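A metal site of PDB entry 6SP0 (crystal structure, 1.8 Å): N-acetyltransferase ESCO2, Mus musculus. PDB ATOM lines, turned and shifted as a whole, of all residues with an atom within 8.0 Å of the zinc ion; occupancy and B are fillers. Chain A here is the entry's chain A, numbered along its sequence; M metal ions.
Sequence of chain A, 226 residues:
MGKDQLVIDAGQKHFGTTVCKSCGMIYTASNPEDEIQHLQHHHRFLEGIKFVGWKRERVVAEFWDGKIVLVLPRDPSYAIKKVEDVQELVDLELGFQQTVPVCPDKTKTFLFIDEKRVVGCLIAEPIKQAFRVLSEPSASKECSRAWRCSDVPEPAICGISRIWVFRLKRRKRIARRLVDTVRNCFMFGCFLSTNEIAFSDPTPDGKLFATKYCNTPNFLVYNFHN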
ATOM      1  N   VAL A  19       4.272 -23.430 -12.168  1.00  0.00           N
ATOM      2  CA  VAL A  19       4.758 -22.614 -13.292  1.00  0.00           C
ATOM      3  C   VAL A  19       5.038 -21.223 -12.761  1.00  0.00           C
ATOM      4  O   VAL A  19       4.115 -20.540 -12.293  1.00  0.00           O
ATOM      5  CB  VAL A  19       3.753 -22.561 -14.448  1.00  0.00           C
ATOM      6  CG1 VAL A  19       4.337 -21.748 -15.609  1.00  0.00           C
ATOM      7  CG2 VAL A  19       3.372 -23.960 -14.888  1.00  0.00           C
ATOM      8  N   CYS A  20       6.281 -20.780 -12.844  1.00  0.00           N
ATOM      9  CA  CYS A  20       6.575 -19.401 -12.461  1.00  0.00           C
ATOM     10  C   CYS A  20       6.016 -18.458 -13.507  1.00  0.00           C
ATOM     11  O   CYS A  20       6.391 -18.559 -14.688  1.00  0.00           O
ATOM     12  CB  CYS A  20       8.076 -19.167 -12.296  1.00  0.00           C
ATOM     13  SG  CYS A  20       8.458 -17.412 -11.964  1.00  0.00           S
ATOM     14  N   LYS A  21       5.141 -17.533 -13.094  1.00  0.00           N
ATOM     15  CA  LYS A  21       4.513 -16.653 -14.066  1.00  0.00           C
ATOM     16  C   LYS A  21       5.498 -15.690 -14.700  1.00  0.00           C
ATOM     17  O   LYS A  21       5.227 -15.187 -15.798  1.00  0.00           O
ATOM     18  CB  LYS A  21       3.392 -15.852 -13.392  1.00  0.00           C
ATOM     19  CG  LYS A  21       2.087 -16.625 -13.237  1.00  0.00           C
ATOM     20  N   SER A  22       6.647 -15.450 -14.074  1.00  0.00           N
ATOM     21  CA  SER A  22       7.546 -14.421 -14.573  1.00  0.00           C
ATOM     22  C   SER A  22       8.713 -14.966 -15.405  1.00  0.00           C
ATOM     23  O   SER A  22       9.130 -14.328 -16.377  1.00  0.00           O
ATOM     24  CB  SER A  22       8.067 -13.588 -13.400  1.00  0.00           C
ATOM     25  OG  SER A  22       9.108 -12.741 -13.838  1.00  0.00           O
ATOM     26  N   CYS A  23       9.273 -16.133 -15.088  1.00  0.00           N
ATOM     27  CA  CYS A  23      10.291 -16.642 -15.994  1.00  0.00           C
ATOM     28  C   CYS A  23       9.819 -17.847 -16.791  1.00  0.00           C
ATOM     29  O   CYS A  23      10.581 -18.353 -17.647  1.00  0.00           O
ATOM     30  CB  CYS A  23      11.550 -17.000 -15.176  1.00  0.00           C
ATOM     31  SG  CYS A  23      11.347 -18.494 -14.157  1.00  0.00           S
ATOM     32  N   GLY A  24       8.608 -18.340 -16.528  1.00  0.00           N
ATOM     33  CA  GLY A  24       8.041 -19.459 -17.239  1.00  0.00           C
ATOM     34  C   GLY A  24       8.545 -20.820 -16.816  1.00  0.00           C
ATOM     35  O   GLY A  24       8.150 -21.834 -17.423  1.00  0.00           O
ATOM     36  N   MET A  25       9.390 -20.900 -15.790  1.00  0.00           N
ATOM     37  CA  MET A  25       9.958 -22.210 -15.470  1.00  0.00           C
ATOM     38  C   MET A  25       8.895 -23.119 -14.868  1.00  0.00           C
ATOM     39  O   MET A  25       8.051 -22.673 -14.090  1.00  0.00           O
ATOM     40  CB  MET A  25      11.132 -22.108 -14.512  1.00  0.00           C
ATOM     41  CG  MET A  25      11.968 -23.408 -14.557  1.00  0.00           C
ATOM     42  SD  MET A  25      13.157 -23.439 -13.225  1.00  0.00           S
ATOM     43  CE  MET A  25      14.472 -24.455 -13.954  1.00  0.00           C
ATOM     44  N   ILE A  26       8.927 -24.380 -15.273  1.00  0.00           N
ATOM     45  CA  ILE A  26       8.048 -25.415 -14.748  1.00  0.00           C
ATOM     46  C   ILE A  26       8.887 -26.300 -13.834  1.00  0.00           C
ATOM     47  O   ILE A  26       9.917 -26.843 -14.244  1.00  0.00           O
ATOM     48  CB  ILE A  26       7.430 -26.244 -15.883  1.00  0.00           C
ATOM     49  CG1 ILE A  26       6.601 -25.335 -16.779  1.00  0.00           C
ATOM     50  CG2 ILE A  26       6.588 -27.394 -15.301  1.00  0.00           C
ATOM     51  CD1 ILE A  26       6.223 -26.002 -18.081  1.00  0.00           C
ATOM     52  N   TYR A  27       8.436 -26.449 -12.591  1.00  0.00           N
ATOM     53  CA  TYR A  27       9.239 -27.160 -11.602  1.00  0.00           C
ATOM     54  C   TYR A  27       8.328 -27.592 -10.469  1.00  0.00           C
ATOM     55  O   TYR A  27       7.142 -27.243 -10.445  1.00  0.00           O
ATOM     56  CB  TYR A  27      10.393 -26.295 -11.074  1.00  0.00           C
ATOM     57  CG  TYR A  27       9.914 -25.091 -10.294  1.00  0.00           C
ATOM     58  CD1 TYR A  27       9.928 -25.082  -8.896  1.00  0.00           C
ATOM     59  CD2 TYR A  27       9.442 -23.983 -10.955  1.00  0.00           C
ATOM     60  CE1 TYR A  27       9.467 -23.975  -8.179  1.00  0.00           C
ATOM     61  CE2 TYR A  27       8.977 -22.867 -10.247  1.00  0.00           C
ATOM     62  CZ  TYR A  27       9.002 -22.874  -8.862  1.00  0.00           C
ATOM     63  OH  TYR A  27       8.553 -21.763  -8.180  1.00  0.00           O
ATOM     64  N   GLU A  35      13.541 -25.660  -5.836  1.00  0.00           N
ATOM     65  CA  GLU A  35      13.355 -24.260  -5.529  1.00  0.00           C
ATOM     66  C   GLU A  35      14.668 -23.497  -5.665  1.00  0.00           C
ATOM     67  O   GLU A  35      14.677 -22.352  -6.119  1.00  0.00           O
ATOM     68  CB  GLU A  35      12.731 -24.087  -4.137  1.00  0.00           C
ATOM     69  CG  GLU A  35      11.971 -22.761  -3.990  1.00  0.00           C
ATOM     70  CD  GLU A  35      10.506 -22.820  -4.463  1.00  0.00           C
ATOM     71  OE1 GLU A  35       9.725 -23.613  -3.892  1.00  0.00           O
ATOM     72  OE2 GLU A  35      10.136 -22.059  -5.398  1.00  0.00           O
ATOM     73  N   GLN A  37      17.106 -24.297  -7.775  1.00  0.00           N
ATOM     74  CA  GLN A  37      17.416 -24.251  -9.193  1.00  0.00           C
ATOM     75  C   GLN A  37      16.493 -23.291  -9.920  1.00  0.00           C
ATOM     76  O   GLN A  37      16.917 -22.590 -10.845  1.00  0.00           O
ATOM     77  CB  GLN A  37      17.340 -25.659  -9.779  1.00  0.00           C
ATOM     78  CG  GLN A  37      18.497 -26.560  -9.306  1.00  0.00           C
ATOM     79  CD  GLN A  37      19.816 -26.252  -9.997  1.00  0.00           C
ATOM     80  OE1 GLN A  37      19.839 -25.846 -11.173  1.00  0.00           O
ATOM     81  NE2 GLN A  37      20.922 -26.450  -9.299  1.00  0.00           N
ATOM     82  N   HIS A  38      15.239 -23.200  -9.481  1.00  0.00           N
ATOM     83  CA  HIS A  38      14.383 -22.175 -10.064  1.00  0.00           C
ATOM     84  C   HIS A  38      14.905 -20.788  -9.704  1.00  0.00           C
ATOM     85  O   HIS A  38      14.962 -19.896 -10.566  1.00  0.00           O
ATOM     86  CB  HIS A  38      12.932 -22.324  -9.603  1.00  0.00           C
ATOM     87  CG  HIS A  38      12.122 -21.090  -9.863  1.00  0.00           C
ATOM     88  ND1 HIS A  38      11.542 -20.345  -8.860  1.00  0.00           N
ATOM     89  CD2 HIS A  38      11.846 -20.432 -11.018  1.00  0.00           C
ATOM     90  CE1 HIS A  38      10.944 -19.295  -9.380  1.00  0.00           C
ATOM     91  NE2 HIS A  38      11.101 -19.324 -10.689  1.00  0.00           N
ATOM     92  N   LEU A  39      15.273 -20.567  -8.444  1.00  0.00           N
ATOM     93  CA  LEU A  39      15.835 -19.273  -8.070  1.00  0.00           C
ATOM     94  C   LEU A  39      16.957 -18.843  -9.033  1.00  0.00           C
ATOM     95  O   LEU A  39      16.967 -17.716  -9.538  1.00  0.00           O
ATOM     96  CB  LEU A  39      16.353 -19.370  -6.632  1.00  0.00           C
ATOM     97  CG  LEU A  39      16.546 -18.072  -5.855  1.00  0.00           C
ATOM     98  CD1 LEU A  39      15.217 -17.327  -5.806  1.00  0.00           C
ATOM     99  CD2 LEU A  39      17.068 -18.416  -4.449  1.00  0.00           C
ATOM    100  N   GLN A  40      17.898 -19.735  -9.300  1.00  0.00           N
ATOM    101  CA  GLN A  40      19.020 -19.391 -10.156  1.00  0.00           C
ATOM    102  C   GLN A  40      18.588 -19.239 -11.620  1.00  0.00           C
ATOM    103  O   GLN A  40      19.077 -18.363 -12.342  1.00  0.00           O
ATOM    104  CB  GLN A  40      20.116 -20.444  -9.961  1.00  0.00           C
ATOM    105  CG  GLN A  40      20.840 -20.173  -8.615  1.00  0.00           C
ATOM    106  CD  GLN A  40      21.521 -21.371  -7.946  1.00  0.00           C
ATOM    107  OE1 GLN A  40      21.525 -22.512  -8.452  1.00  0.00           O
ATOM    108  NE2 GLN A  40      22.138 -21.103  -6.788  1.00  0.00           N
ATOM    109  N   HIS A  41      17.660 -20.078 -12.087  1.00  0.00           N
ATOM    110  CA  HIS A  41      17.205 -19.956 -13.472  1.00  0.00           C
ATOM    111  C   HIS A  41      16.444 -18.660 -13.655  1.00  0.00           C
ATOM    112  O   HIS A  41      16.630 -17.948 -14.649  1.00  0.00           O
ATOM    113  CB  HIS A  41      16.327 -21.157 -13.844  1.00  0.00           C
ATOM    114  CG  HIS A  41      15.650 -21.023 -15.167  1.00  0.00           C
ATOM    115  ND1 HIS A  41      16.144 -21.610 -16.320  1.00  0.00           N
ATOM    116  CD2 HIS A  41      14.505 -20.402 -15.529  1.00  0.00           C
ATOM    117  CE1 HIS A  41      15.329 -21.346 -17.330  1.00  0.00           C
ATOM    118  NE2 HIS A  41      14.334 -20.609 -16.875  1.00  0.00           N
ATOM    119  N   HIS A  42      15.550 -18.368 -12.712  1.00  0.00           N
ATOM    120  CA  HIS A  42      14.777 -17.135 -12.661  1.00  0.00           C
ATOM    121  C   HIS A  42      15.680 -15.910 -12.774  1.00  0.00           C
ATOM    122  O   HIS A  42      15.415 -15.002 -13.579  1.00  0.00           O
ATOM    123  CB  HIS A  42      13.994 -17.167 -11.341  1.00  0.00           C
ATOM    124  CG  HIS A  42      13.022 -16.052 -11.158  1.00  0.00           C
ATOM    125  ND1 HIS A  42      11.670 -16.203 -11.399  1.00  0.00           N
ATOM    126  CD2 HIS A  42      13.199 -14.790 -10.696  1.00  0.00           C
ATOM    127  CE1 HIS A  42      11.061 -15.070 -11.099  1.00  0.00           C
ATOM    128  NE2 HIS A  42      11.963 -14.194 -10.689  1.00  0.00           N
ATOM    129  N   HIS A  43      16.774 -15.896 -12.030  1.00  0.00           N
ATOM    130  CA  HIS A  43      17.700 -14.751 -12.063  1.00  0.00           C
ATOM    131  C   HIS A  43      18.341 -14.578 -13.443  1.00  0.00           C
ATOM    132  O   HIS A  43      18.388 -13.462 -13.978  1.00  0.00           O
ATOM    133  CB  HIS A  43      18.784 -14.915 -10.997  1.00  0.00           C
ATOM    134  CG  HIS A  43      19.832 -13.851 -11.061  1.00  0.00           C
ATOM    135  ND1 HIS A  43      21.075 -14.065 -11.616  1.00  0.00           N
ATOM    136  CD2 HIS A  43      19.805 -12.547 -10.670  1.00  0.00           C
ATOM    137  CE1 HIS A  43      21.779 -12.940 -11.545  1.00  0.00           C
ATOM    138  NE2 HIS A  43      21.031 -12.007 -10.980  1.00  0.00           N
ATOM    139  N   PHE A  45      17.332 -15.640 -16.298  1.00  0.00           N
ATOM    140  CA  PHE A  45      16.334 -15.351 -17.320  1.00  0.00           C
ATOM    141  C   PHE A  45      15.899 -13.895 -17.268  1.00  0.00           C
ATOM    142  O   PHE A  45      15.888 -13.212 -18.300  1.00  0.00           O
ATOM    143  CB  PHE A  45      15.127 -16.284 -17.165  1.00  0.00           C
ATOM    144  CG  PHE A  45      14.259 -16.317 -18.377  1.00  0.00           C
ATOM    145  CD1 PHE A  45      13.252 -15.419 -18.518  1.00  0.00           C
ATOM    146  CD2 PHE A  45      14.516 -17.240 -19.398  1.00  0.00           C
ATOM    147  CE1 PHE A  45      12.440 -15.429 -19.663  1.00  0.00           C
ATOM    148  CE2 PHE A  45      13.719 -17.267 -20.546  1.00  0.00           C
ATOM    149  CZ  PHE A  45      12.668 -16.340 -20.665  1.00  0.00           C
ATOM    150  N   LEU A  46      15.528 -13.401 -16.074  1.00  0.00           N
ATOM    151  CA  LEU A  46      15.026 -12.026 -15.958  1.00  0.00           C
ATOM    152  C   LEU A  46      16.105 -11.007 -16.289  1.00  0.00           C
ATOM    153  O   LEU A  46      15.796  -9.943 -16.838  1.00  0.00           O
ATOM    154  CB  LEU A  46      14.481 -11.781 -14.560  1.00  0.00           C
ATOM    155  CG  LEU A  46      13.160 -12.449 -14.249  1.00  0.00           C
ATOM    156  CD1 LEU A  46      12.559 -11.767 -13.040  1.00  0.00           C
ATOM    157  CD2 LEU A  46      12.240 -12.361 -15.451  1.00  0.00           C
HETATM  158 ZN    ZN M   1      10.714 -17.799 -12.045  1.00  0.00          ZN
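Within 4 Å of the zinc ion: Cys 20, Cys 23, His 38 and His 42.
The zinc ion is bound by ND1 of His 42 (2.0 Å).
A ring nitrogen (NE2) of His 38 binds the zinc ion.
The side-chain sulfur (SG) of Cys 20 is bound to the zinc ion.
SG of Cys 23 binds the zinc ion (2.3 Å).
O of Met 25 lies within hydrogen-bond range of N of Cys 20 (2.9 Å).
SG of Cys 20 lies close to N of Ser 22.
The backbone NH (N) of Met 25 sits close to the side-chain sulfur (SG) of Cys 23 (3.5 Å).
The side-chain hydroxyl of Tyr 27 is in hydrogen-bond range of a ring nitrogen (ND1) of His 38 (3.4 Å).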
